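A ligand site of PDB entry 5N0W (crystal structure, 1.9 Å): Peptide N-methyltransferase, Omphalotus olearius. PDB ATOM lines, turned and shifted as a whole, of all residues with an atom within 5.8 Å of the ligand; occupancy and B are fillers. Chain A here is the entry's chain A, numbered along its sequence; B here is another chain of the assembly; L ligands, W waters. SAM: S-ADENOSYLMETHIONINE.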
ATOM      1  N   ILE A  18      -8.693   6.804  -1.495  1.00  0.00           N
ATOM      2  CA  ILE A  18      -9.395   5.531  -1.702  1.00  0.00           C
ATOM      3  C   ILE A  18     -10.084   5.490  -3.042  1.00  0.00           C
ATOM      4  O   ILE A  18      -9.941   4.498  -3.784  1.00  0.00           O
ATOM      5  CB  ILE A  18     -10.361   5.243  -0.556  1.00  0.00           C
ATOM      6  CG1 ILE A  18      -9.570   5.091   0.745  1.00  0.00           C
ATOM      7  CG2 ILE A  18     -11.196   3.984  -0.836  1.00  0.00           C
ATOM      8  CD1 ILE A  18      -8.607   3.912   0.823  1.00  0.00           C
ATOM      9  N   ILE A  43      -4.519  -0.376  -5.617  1.00  0.00           N
ATOM     10  CA  ILE A  43      -5.393  -1.513  -5.893  1.00  0.00           C
ATOM     11  C   ILE A  43      -6.481  -1.273  -6.936  1.00  0.00           C
ATOM     12  O   ILE A  43      -7.345  -2.145  -7.130  1.00  0.00           O
ATOM     13  CB  ILE A  43      -5.958  -2.161  -4.608  1.00  0.00           C
ATOM     14  CG1 ILE A  43      -6.828  -1.208  -3.801  1.00  0.00           C
ATOM     15  CG2 ILE A  43      -4.824  -2.685  -3.734  1.00  0.00           C
ATOM     16  CD1 ILE A  43      -7.549  -1.916  -2.673  1.00  0.00           C
ATOM     17  N   TYR A  97      -1.908   3.328  -1.613  1.00  0.00           N
ATOM     18  CA  TYR A  97      -3.289   3.766  -1.676  1.00  0.00           C
ATOM     19  C   TYR A  97      -3.809   4.204  -0.277  1.00  0.00           C
ATOM     20  O   TYR A  97      -3.351   3.728   0.757  1.00  0.00           O
ATOM     21  CB  TYR A  97      -4.214   2.749  -2.352  1.00  0.00           C
ATOM     22  CG  TYR A  97      -4.648   1.626  -1.490  1.00  0.00           C
ATOM     23  CD1 TYR A  97      -3.868   0.491  -1.346  1.00  0.00           C
ATOM     24  CD2 TYR A  97      -5.882   1.686  -0.843  1.00  0.00           C
ATOM     25  CE1 TYR A  97      -4.290  -0.575  -0.557  1.00  0.00           C
ATOM     26  CE2 TYR A  97      -6.306   0.640  -0.044  1.00  0.00           C
ATOM     27  CZ  TYR A  97      -5.509  -0.490   0.083  1.00  0.00           C
ATOM     28  OH  TYR A  97      -5.918  -1.535   0.873  1.00  0.00           O
ATOM     29  N   GLY A  98      -4.719   5.159  -0.293  1.00  0.00           N
ATOM     30  CA  GLY A  98      -5.301   5.707   0.923  1.00  0.00           C
ATOM     31  C   GLY A  98      -4.306   6.673   1.520  1.00  0.00           C
ATOM     32  O   GLY A  98      -3.782   7.512   0.821  1.00  0.00           O
ATOM     33  N   HIS A  99      -4.069   6.533   2.817  1.00  0.00           N
ATOM     34  CA  HIS A  99      -3.083   7.285   3.581  1.00  0.00           C
ATOM     35  C   HIS A  99      -1.933   6.282   3.684  1.00  0.00           C
ATOM     36  O   HIS A  99      -2.177   5.130   4.096  1.00  0.00           O
ATOM     37  CB  HIS A  99      -3.634   7.580   4.974  1.00  0.00           C
ATOM     38  CG  HIS A  99      -2.733   8.365   5.873  1.00  0.00           C
ATOM     39  ND1 HIS A  99      -1.431   7.997   6.156  1.00  0.00           N
ATOM     40  CD2 HIS A  99      -2.986   9.464   6.634  1.00  0.00           C
ATOM     41  CE1 HIS A  99      -0.908   8.843   7.027  1.00  0.00           C
ATOM     42  NE2 HIS A  99      -1.830   9.755   7.324  1.00  0.00           N
ATOM     43  N   PRO A 100      -0.693   6.697   3.362  1.00  0.00           N
ATOM     44  CA  PRO A 100       0.415   5.719   3.246  1.00  0.00           C
ATOM     45  C   PRO A 100       0.951   5.178   4.543  1.00  0.00           C
ATOM     46  O   PRO A 100       1.819   4.304   4.534  1.00  0.00           O
ATOM     47  CB  PRO A 100       1.494   6.518   2.527  1.00  0.00           C
ATOM     48  CG  PRO A 100       1.243   7.930   2.898  1.00  0.00           C
ATOM     49  CD  PRO A 100      -0.258   8.034   2.926  1.00  0.00           C
ATOM     50  N   GLY A 101       0.455   5.705   5.664  1.00  0.00           N
ATOM     51  CA  GLY A 101       0.879   5.292   6.989  1.00  0.00           C
ATOM     52  C   GLY A 101      -0.228   4.704   7.836  1.00  0.00           C
ATOM     53  O   GLY A 101      -0.023   4.511   9.013  1.00  0.00           O
ATOM     54  N   VAL A 102      -1.375   4.437   7.237  1.00  0.00           N
ATOM     55  CA  VAL A 102      -2.534   3.874   7.919  1.00  0.00           C
ATOM     56  C   VAL A 102      -2.701   2.424   7.477  1.00  0.00           C
ATOM     57  O   VAL A 102      -3.081   2.154   6.332  1.00  0.00           O
ATOM     58  CB  VAL A 102      -3.781   4.725   7.604  1.00  0.00           C
ATOM     59  CG1 VAL A 102      -5.068   4.059   8.057  1.00  0.00           C
ATOM     60  CG2 VAL A 102      -3.630   6.100   8.264  1.00  0.00           C
ATOM     61  N   PHE A 103      -2.437   1.499   8.400  1.00  0.00           N
ATOM     62  CA  PHE A 103      -2.432   0.064   8.130  1.00  0.00           C
ATOM     63  C   PHE A 103      -1.531  -0.285   6.941  1.00  0.00           C
ATOM     64  O   PHE A 103      -1.969  -0.941   6.007  1.00  0.00           O
ATOM     65  CB  PHE A 103      -3.876  -0.441   7.904  1.00  0.00           C
ATOM     66  CG  PHE A 103      -4.746  -0.345   9.126  1.00  0.00           C
ATOM     67  CD1 PHE A 103      -5.182   0.891   9.583  1.00  0.00           C
ATOM     68  CD2 PHE A 103      -5.115  -1.474   9.839  1.00  0.00           C
ATOM     69  CE1 PHE A 103      -5.973   1.019  10.721  1.00  0.00           C
ATOM     70  CE2 PHE A 103      -5.891  -1.342  10.994  1.00  0.00           C
ATOM     71  CZ  PHE A 103      -6.333  -0.102  11.429  1.00  0.00           C
ATOM     72  N   VAL A 104      -0.273   0.205   6.971  1.00  0.00           N
ATOM     73  CA  VAL A 104       0.740  -0.061   5.930  1.00  0.00           C
ATOM     74  C   VAL A 104       2.063  -0.330   6.644  1.00  0.00           C
ATOM     75  O   VAL A 104       2.425   0.439   7.506  1.00  0.00           O
ATOM     76  CB  VAL A 104       0.933   1.160   4.982  1.00  0.00           C
ATOM     77  CG1 VAL A 104       2.051   0.912   3.980  1.00  0.00           C
ATOM     78  CG2 VAL A 104      -0.346   1.504   4.244  1.00  0.00           C
ATOM     79  N   VAL A 127      -6.002  10.609   2.337  1.00  0.00           N
ATOM     80  CA  VAL A 127      -7.336  10.187   2.751  1.00  0.00           C
ATOM     81  C   VAL A 127      -7.392   8.673   2.982  1.00  0.00           C
ATOM     82  O   VAL A 127      -7.210   7.892   2.033  1.00  0.00           O
ATOM     83  CB  VAL A 127      -8.378  10.588   1.690  1.00  0.00           C
ATOM     84  CG1 VAL A 127      -9.745   9.970   1.962  1.00  0.00           C
ATOM     85  CG2 VAL A 127      -8.480  12.113   1.593  1.00  0.00           C
ATOM     86  N   SER A 128      -7.670   8.256   4.213  1.00  0.00           N
ATOM     87  CA  SER A 128      -7.779   6.834   4.545  1.00  0.00           C
ATOM     88  C   SER A 128      -9.196   6.300   4.344  1.00  0.00           C
ATOM     89  O   SER A 128     -10.157   7.068   4.163  1.00  0.00           O
ATOM     90  CB  SER A 128      -7.388   6.590   6.000  1.00  0.00           C
ATOM     91  OG  SER A 128      -8.365   7.140   6.867  1.00  0.00           O
ATOM     92  N   ALA A 129      -9.310   4.978   4.453  1.00  0.00           N
ATOM     93  CA  ALA A 129     -10.619   4.310   4.444  1.00  0.00           C
ATOM     94  C   ALA A 129     -11.449   4.755   5.634  1.00  0.00           C
ATOM     95  O   ALA A 129     -12.663   4.887   5.513  1.00  0.00           O
ATOM     96  CB  ALA A 129     -10.450   2.799   4.447  1.00  0.00           C
ATOM     97  N   GLU A 130     -10.810   5.034   6.774  1.00  0.00           N
ATOM     98  CA  GLU A 130     -11.510   5.597   7.909  1.00  0.00           C
ATOM     99  C   GLU A 130     -12.090   7.003   7.615  1.00  0.00           C
ATOM    100  O   GLU A 130     -13.231   7.292   7.961  1.00  0.00           O
ATOM    101  CB  GLU A 130     -10.646   5.595   9.170  1.00  0.00           C
ATOM    102  CG  GLU A 130     -11.419   6.065  10.394  1.00  0.00           C
ATOM    103  CD  GLU A 130     -10.761   5.731  11.720  1.00  0.00           C
ATOM    104  OE1 GLU A 130     -11.130   4.681  12.280  1.00  0.00           O
ATOM    105  OE2 GLU A 130      -9.891   6.487  12.184  1.00  0.00           O
ATOM    106  N   LEU A 169     -13.244  -1.372  12.790  1.00  0.00           N
ATOM    107  CA  LEU A 169     -12.360  -2.513  12.580  1.00  0.00           C
ATOM    108  C   LEU A 169     -11.974  -2.676  11.106  1.00  0.00           C
ATOM    109  O   LEU A 169     -12.842  -2.935  10.260  1.00  0.00           O
ATOM    110  CB  LEU A 169     -13.027  -3.802  13.053  1.00  0.00           C
ATOM    111  CG  LEU A 169     -13.446  -3.836  14.529  1.00  0.00           C
ATOM    112  CD1 LEU A 169     -14.159  -5.138  14.843  1.00  0.00           C
ATOM    113  CD2 LEU A 169     -12.243  -3.660  15.419  1.00  0.00           C
ATOM    114  N   PHE A 170     -10.682  -2.542  10.829  1.00  0.00           N
ATOM    115  CA  PHE A 170     -10.101  -2.796   9.516  1.00  0.00           C
ATOM    116  C   PHE A 170      -9.776  -4.294   9.386  1.00  0.00           C
ATOM    117  O   PHE A 170      -9.603  -4.980  10.382  1.00  0.00           O
ATOM    118  CB  PHE A 170      -8.769  -2.069   9.367  1.00  0.00           C
ATOM    119  CG  PHE A 170      -8.867  -0.599   9.043  1.00  0.00           C
ATOM    120  CD1 PHE A 170      -9.493   0.290   9.919  1.00  0.00           C
ATOM    121  CD2 PHE A 170      -8.245  -0.089   7.905  1.00  0.00           C
ATOM    122  CE1 PHE A 170      -9.540   1.660   9.625  1.00  0.00           C
ATOM    123  CE2 PHE A 170      -8.280   1.272   7.620  1.00  0.00           C
ATOM    124  CZ  PHE A 170      -8.939   2.144   8.482  1.00  0.00           C
ATOM    125  N   GLN A 171      -9.663  -4.767   8.143  1.00  0.00           N
ATOM    126  CA  GLN A 171      -9.180  -6.146   7.862  1.00  0.00           C
ATOM    127  C   GLN A 171     -10.052  -7.229   8.463  1.00  0.00           C
ATOM    128  O   GLN A 171      -9.566  -8.299   8.831  1.00  0.00           O
ATOM    129  CB  GLN A 171      -7.700  -6.303   8.265  1.00  0.00           C
ATOM    130  CG  GLN A 171      -6.881  -5.173   7.677  1.00  0.00           C
ATOM    131  CD  GLN A 171      -5.422  -5.452   7.505  1.00  0.00           C
ATOM    132  OE1 GLN A 171      -4.792  -4.838   6.652  1.00  0.00           O
ATOM    133  NE2 GLN A 171      -4.866  -6.324   8.325  1.00  0.00           N
ATOM    134  N   VAL A 172     -11.355  -6.966   8.511  1.00  0.00           N
ATOM    135  CA  VAL A 172     -12.343  -7.964   8.940  1.00  0.00           C
ATOM    136  C   VAL A 172     -12.509  -9.132   7.949  1.00  0.00           C
ATOM    137  O   VAL A 172     -13.063 -10.168   8.304  1.00  0.00           O
ATOM    138  CB  VAL A 172     -13.724  -7.332   9.214  1.00  0.00           C
ATOM    139  CG1 VAL A 172     -13.640  -6.372  10.396  1.00  0.00           C
ATOM    140  CG2 VAL A 172     -14.290  -6.621   7.981  1.00  0.00           C
ATOM    141  N   GLY A 173     -12.046  -8.952   6.706  1.00  0.00           N
ATOM    142  CA  GLY A 173     -12.042 -10.010   5.718  1.00  0.00           C
ATOM    143  C   GLY A 173     -10.873 -10.983   5.739  1.00  0.00           C
ATOM    144  O   GLY A 173     -10.846 -11.903   4.932  1.00  0.00           O
ATOM    145  N   CYS A 174      -9.909 -10.792   6.638  1.00  0.00           N
ATOM    146  CA  CYS A 174      -8.765 -11.686   6.736  1.00  0.00           C
ATOM    147  C   CYS A 174      -8.340 -11.965   8.181  1.00  0.00           C
ATOM    148  O   CYS A 174      -7.168 -11.888   8.549  1.00  0.00           O
ATOM    149  CB  CYS A 174      -7.610 -11.130   5.928  1.00  0.00           C
ATOM    150  SG  CYS A 174      -7.222  -9.421   6.329  1.00  0.00           S
ATOM    151  N   TYR A 210     -18.993  -1.762   5.640  1.00  0.00           N
ATOM    152  CA  TYR A 210     -18.635  -0.579   4.860  1.00  0.00           C
ATOM    153  C   TYR A 210     -17.567  -0.885   3.821  1.00  0.00           C
ATOM    154  O   TYR A 210     -16.505  -1.419   4.163  1.00  0.00           O
ATOM    155  CB  TYR A 210     -18.099   0.532   5.779  1.00  0.00           C
ATOM    156  CG  TYR A 210     -17.657   1.754   5.009  1.00  0.00           C
ATOM    157  CD1 TYR A 210     -18.579   2.489   4.284  1.00  0.00           C
ATOM    158  CD2 TYR A 210     -16.311   2.153   4.967  1.00  0.00           C
ATOM    159  CE1 TYR A 210     -18.190   3.603   3.544  1.00  0.00           C
ATOM    160  CE2 TYR A 210     -15.921   3.274   4.242  1.00  0.00           C
ATOM    161  CZ  TYR A 210     -16.869   3.997   3.540  1.00  0.00           C
ATOM    162  OH  TYR A 210     -16.530   5.121   2.818  1.00  0.00           O
ATOM    163  N   ILE A 211     -17.858  -0.535   2.569  1.00  0.00           N
ATOM    164  CA  ILE A 211     -16.877  -0.524   1.496  1.00  0.00           C
ATOM    165  C   ILE A 211     -17.021   0.814   0.755  1.00  0.00           C
ATOM    166  O   ILE A 211     -18.055   1.057   0.125  1.00  0.00           O
ATOM    167  CB  ILE A 211     -17.038  -1.679   0.478  1.00  0.00           C
ATOM    168  CG1 ILE A 211     -16.974  -3.051   1.166  1.00  0.00           C
ATOM    169  CG2 ILE A 211     -15.916  -1.632  -0.576  1.00  0.00           C
ATOM    170  CD1 ILE A 211     -17.404  -4.201   0.270  1.00  0.00           C
ATOM    171  N   ALA A 212     -16.005   1.666   0.866  1.00  0.00           N
ATOM    172  CA  ALA A 212     -15.961   2.910   0.104  1.00  0.00           C
ATOM    173  C   ALA A 212     -15.909   2.597  -1.388  1.00  0.00           C
ATOM    174  O   ALA A 212     -15.216   1.661  -1.793  1.00  0.00           O
ATOM    175  CB  ALA A 212     -14.746   3.756   0.493  1.00  0.00           C
ATOM    176  N   ALA A 213     -16.648   3.374  -2.173  1.00  0.00           N
ATOM    177  CA  ALA A 213     -16.547   3.327  -3.621  1.00  0.00           C
ATOM    178  C   ALA A 213     -15.090   3.581  -4.036  1.00  0.00           C
ATOM    179  O   ALA A 213     -14.451   4.556  -3.599  1.00  0.00           O
ATOM    180  CB  ALA A 213     -17.453   4.373  -4.243  1.00  0.00           C
ATOM    181  N   MET A 214     -14.565   2.680  -4.857  1.00  0.00           N
ATOM    182  CA  MET A 214     -13.224   2.834  -5.418  1.00  0.00           C
ATOM    183  C   MET A 214     -13.215   3.532  -6.779  1.00  0.00           C
ATOM    184  O   MET A 214     -12.245   4.194  -7.101  1.00  0.00           O
ATOM    185  CB  MET A 214     -12.507   1.492  -5.473  1.00  0.00           C
ATOM    186  CG  MET A 214     -12.088   1.017  -4.088  1.00  0.00           C
ATOM    187  SD  MET A 214     -11.468  -0.677  -4.000  1.00  0.00           S
ATOM    188  CE  MET A 214     -10.243  -0.564  -5.295  1.00  0.00           C
ATOM    189  N   GLY A 240     -14.982  -8.993   2.314  1.00  0.00           N
ATOM    190  CA  GLY A 240     -13.758  -9.265   1.577  1.00  0.00           C
ATOM    191  C   GLY A 240     -12.587  -8.408   2.031  1.00  0.00           C
ATOM    192  O   GLY A 240     -12.591  -7.833   3.117  1.00  0.00           O
ATOM    193  N   GLY A 241     -11.592  -8.309   1.159  1.00  0.00           N
ATOM    194  CA  GLY A 241     -10.331  -7.653   1.468  1.00  0.00           C
ATOM    195  C   GLY A 241     -10.369  -6.144   1.643  1.00  0.00           C
ATOM    196  O   GLY A 241      -9.483  -5.590   2.285  1.00  0.00           O
ATOM    197  N   VAL A 242     -11.394  -5.486   1.086  1.00  0.00           N
ATOM    198  CA  VAL A 242     -11.595  -4.034   1.262  1.00  0.00           C
ATOM    199  C   VAL A 242     -12.783  -3.709   2.164  1.00  0.00           C
ATOM    200  O   VAL A 242     -13.274  -2.569   2.153  1.00  0.00           O
ATOM    201  CB  VAL A 242     -11.729  -3.295  -0.094  1.00  0.00           C
ATOM    202  CG1 VAL A 242     -10.379  -3.213  -0.788  1.00  0.00           C
ATOM    203  CG2 VAL A 242     -12.783  -3.917  -0.999  1.00  0.00           C
ATOM    204  N   SER A 243     -13.225  -4.690   2.957  1.00  0.00           N
ATOM    205  CA  SER A 243     -14.285  -4.498   3.943  1.00  0.00           C
ATOM    206  C   SER A 243     -13.737  -3.932   5.268  1.00  0.00           C
ATOM    207  O   SER A 243     -12.697  -4.361   5.767  1.00  0.00           O
ATOM    208  CB  SER A 243     -15.015  -5.815   4.202  1.00  0.00           C
ATOM    209  OG  SER A 243     -15.600  -6.330   3.017  1.00  0.00           O
ATOM    210  N   THR A 244     -14.466  -2.969   5.814  1.00  0.00           N
ATOM    211  CA  THR A 244     -14.251  -2.440   7.152  1.00  0.00           C
ATOM    212  C   THR A 244     -15.583  -2.534   7.877  1.00  0.00           C
ATOM    213  O   THR A 244     -16.632  -2.426   7.248  1.00  0.00           O
ATOM    214  CB  THR A 244     -13.771  -0.987   7.069  1.00  0.00           C
ATOM    215  OG1 THR A 244     -12.481  -0.972   6.456  1.00  0.00           O
ATOM    216  CG2 THR A 244     -13.682  -0.322   8.426  1.00  0.00           C
ATOM    217  N   PRO B 398      -3.431  -6.529  -0.634  1.00  0.00           N
ATOM    218  CA  PRO B 398      -2.417  -6.448   0.424  1.00  0.00           C
ATOM    219  C   PRO B 398      -3.038  -6.167   1.799  1.00  0.00           C
ATOM    220  O   PRO B 398      -4.077  -5.506   1.878  1.00  0.00           O
ATOM    221  CB  PRO B 398      -1.571  -5.249  -0.026  1.00  0.00           C
ATOM    222  CG  PRO B 398      -2.537  -4.343  -0.680  1.00  0.00           C
ATOM    223  CD  PRO B 398      -3.518  -5.251  -1.382  1.00  0.00           C
ATOM    224  N   TRP B 399      -2.404  -6.664   2.865  1.00  0.00           N
ATOM    225  CA  TRP B 399      -2.834  -6.411   4.249  1.00  0.00           C
ATOM    226  C   TRP B 399      -1.656  -5.909   5.087  1.00  0.00           C
ATOM    227  O   TRP B 399      -0.556  -5.716   4.568  1.00  0.00           O
ATOM    228  CB  TRP B 399      -3.497  -7.665   4.841  1.00  0.00           C
ATOM    229  CG  TRP B 399      -2.559  -8.681   5.438  1.00  0.00           C
ATOM    230  CD1 TRP B 399      -2.224  -8.810   6.746  1.00  0.00           C
ATOM    231  CD2 TRP B 399      -1.844  -9.696   4.731  1.00  0.00           C
ATOM    232  NE1 TRP B 399      -1.336  -9.844   6.911  1.00  0.00           N
ATOM    233  CE2 TRP B 399      -1.088 -10.409   5.684  1.00  0.00           C
ATOM    234  CE3 TRP B 399      -1.759 -10.075   3.383  1.00  0.00           C
ATOM    235  CZ2 TRP B 399      -0.253 -11.485   5.339  1.00  0.00           C
ATOM    236  CZ3 TRP B 399      -0.937 -11.148   3.037  1.00  0.00           C
ATOM    237  CH2 TRP B 399      -0.193 -11.841   4.020  1.00  0.00           C
ATOM    238  N   VAL B 400      -1.896  -5.676   6.384  1.00  0.00           N
ATOM    239  CA  VAL B 400      -0.864  -5.206   7.325  1.00  0.00           C
ATOM    240  C   VAL B 400      -0.719  -6.233   8.459  1.00  0.00           C
ATOM    241  O   VAL B 400      -1.710  -6.656   9.056  1.00  0.00           O
ATOM    242  CB  VAL B 400      -1.180  -3.784   7.869  1.00  0.00           C
ATOM    243  CG1 VAL B 400      -2.319  -3.794   8.892  1.00  0.00           C
ATOM    244  CG2 VAL B 400       0.055  -3.123   8.466  1.00  0.00           C
HETATM  245  N   SAM L   1      -3.733   2.679   3.698  1.00  0.00           N
HETATM  246  CA  SAM L   1      -5.113   2.232   3.533  1.00  0.00           C
HETATM  247  C   SAM L   1      -5.999   3.342   4.075  1.00  0.00           C
HETATM  248  O   SAM L   1      -7.187   3.091   4.417  1.00  0.00           O
HETATM  249  OXT SAM L   1      -5.496   4.488   4.199  1.00  0.00           O
HETATM  250  CB  SAM L   1      -5.413   0.904   4.267  1.00  0.00           C
HETATM  251  CG  SAM L   1      -4.542  -0.293   3.838  1.00  0.00           C
HETATM  252  SD  SAM L   1      -4.915  -1.770   4.612  1.00  0.00           S
HETATM  253  CE  SAM L   1      -3.610  -2.770   4.252  1.00  0.00           C
HETATM  254  C5' SAM L   1      -6.320  -2.566   4.044  1.00  0.00           C
HETATM  255  C4' SAM L   1      -7.607  -2.402   4.864  1.00  0.00           C
HETATM  256  O4' SAM L   1      -8.120  -1.081   4.654  1.00  0.00           O
HETATM  257  C3' SAM L   1      -8.795  -3.260   4.452  1.00  0.00           C
HETATM  258  O3' SAM L   1      -8.890  -4.561   5.033  1.00  0.00           O
HETATM  259  C2' SAM L   1      -9.987  -2.425   4.888  1.00  0.00           C
HETATM  260  O2' SAM L   1     -10.274  -2.528   6.276  1.00  0.00           O
HETATM  261  C1' SAM L   1      -9.533  -1.020   4.610  1.00  0.00           C
HETATM  262  N9  SAM L   1      -9.989  -0.619   3.262  1.00  0.00           N
HETATM  263  C8  SAM L   1      -9.258  -0.565   2.131  1.00  0.00           C
HETATM  264  N7  SAM L   1     -10.014  -0.165   1.076  1.00  0.00           N
HETATM  265  C5  SAM L   1     -11.254   0.059   1.564  1.00  0.00           C
HETATM  266  C6  SAM L   1     -12.545   0.495   1.001  1.00  0.00           C
HETATM  267  N6  SAM L   1     -12.653   0.777  -0.318  1.00  0.00           N
HETATM  268  N1  SAM L   1     -13.591   0.603   1.828  1.00  0.00           N
HETATM  269  C2  SAM L   1     -13.503   0.305   3.158  1.00  0.00           C
HETATM  270  N3  SAM L   1     -12.355  -0.118   3.735  1.00  0.00           N
HETATM  271  C4  SAM L   1     -11.230  -0.241   2.994  1.00  0.00           C
HETATM  272  O   HOH W   1      -9.846   0.701  -1.531  1.00  0.00           O
HETATM  273  O   HOH W   2     -11.223  -6.549   5.273  1.00  0.00           O
HETATM  274  O   HOH W   3      -2.325   1.385   1.642  1.00  0.00           O
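An oxygen (O2') of the ligand lies within hydrogen-bond range of the side-chain hydroxyl (OG1) of Thr 244.
The backbone carbonyl oxygen of Val 102 sits at hydrogen-bond distance from a nitrogen (N) of the ligand, at 2.8 Å.
The backbone NH of Ala 212 lies within hydrogen-bond range of a nitrogen (N1) of the ligand, 2.8 Å away.
A nitrogen (N6) of the ligand is in hydrogen-bond range of the backbone carbonyl oxygen (O) of Ala 212, at 3.1 Å.
The backbone NH (N) of Ala 129 sits at hydrogen-bond distance from an oxygen (O) of the ligand, 2.8 Å away.
N of His 99 sits at hydrogen-bond distance from OXT of the ligand, at 2.9 Å.
N of the ligand lies within hydrogen-bond range of O of His 99.
N of Gln 171 is in hydrogen-bond range of O2' of the ligand (3.0 Å).
An oxygen (O3') of the ligand lies within hydrogen-bond range of the backbone carbonyl oxygen (O) of Gly 241, 3.0 Å away.
An oxygen (O2') of the ligand sits at hydrogen-bond distance from the backbone carbonyl oxygen of Ser 243, 3.1 Å away.
A nitrogen (N) of the ligand sits at hydrogen-bond distance from the backbone carbonyl oxygen (O) of Tyr 97 (3.1 Å).
The backbone NH (N) of Tyr 210 is in hydrogen-bond range of the backbone carbonyl oxygen (O) of Thr 244, at 2.9 Å.
The backbone NH of Gly 101 lies within hydrogen-bond range of a ring nitrogen (ND1) of His 99, at 3.0 Å.
The side-chain amide oxygen of Gln 171 is in hydrogen-bond range of the backbone NH of Val 400 of chain B.
The backbone carbonyl oxygen (O) of Gln 171 sits at hydrogen-bond distance from the side-chain sulfur (SG) of Cys 174, at 3.6 Å.
The backbone NH (N) of Gly 240 is in hydrogen-bond range of the side-chain hydroxyl (OG) of Ser 243 (2.8 Å).
The side-chain hydroxyl of Ser 128 sits close to the backbone NH of Glu 130, at 3.2 Å.
Water W1 bridges a nitrogen (N7) of the ligand (2.8 Å) and the side-chain sulfur (SD) of Met 214 (3.3 Å).
Water W3 lies within hydrogen-bond range of O of Tyr 97 (2.7 Å) and N of the ligand (2.8 Å).
Water W2 lies within hydrogen-bond range of O of Ser 243, O of Gly 240, N of Gly 173, O3' of the ligand and N of Val 172.
A sulfur (SD) of the ligand lies close to the backbone carbonyl oxygen of Phe 103 (3.4 Å).
The backbone carbonyl oxygen of Val 242 sits close to a nitrogen (N3) of the ligand (3.1 Å).
CG2 of Ile 18 touches N6 of the ligand (3.6 Å).
CA of Gly 98 touches OXT of the ligand (3.5 Å).
Val 104 touches the ligand (CG2 to N, 3.6 Å).
Ser 128 touches the ligand.
CA of Phe 170 touches O2' of the ligand, 3.3 Å away.
Tyr 210 touches the ligand.
Ile 211 touches the ligand.
CG of Met 214 touches N6 of the ligand, 3.8 Å away.
Pro 398 of chain B touches the ligand.
Trp 399 of chain B touches the ligand (CA to CE, 3.7 Å).
N of Val 400 of chain B touches CE of the ligand, at 3.99 Å.
Hydrophobic or aromatic side chains that line the ligand: Ile 18, Tyr 97, His 99, Val 102, Phe 103, Val 104, Ala 129, Phe 170, Tyr 210, Ala 212, Met 214 and Val 242.
Within 4 Å of the ligand: Ile 18, Tyr 97, Gly 98, His 99, Val 102, Phe 103, Val 104, Ser 128, Ala 129, Phe 170, Gln 171, Tyr 210, Ile 211, Ala 212, Met 214, Gly 241, Val 242, Ser 243, Thr 244, Pro 398 of chain B, Trp 399 of chain B and Val 400 of chain B.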
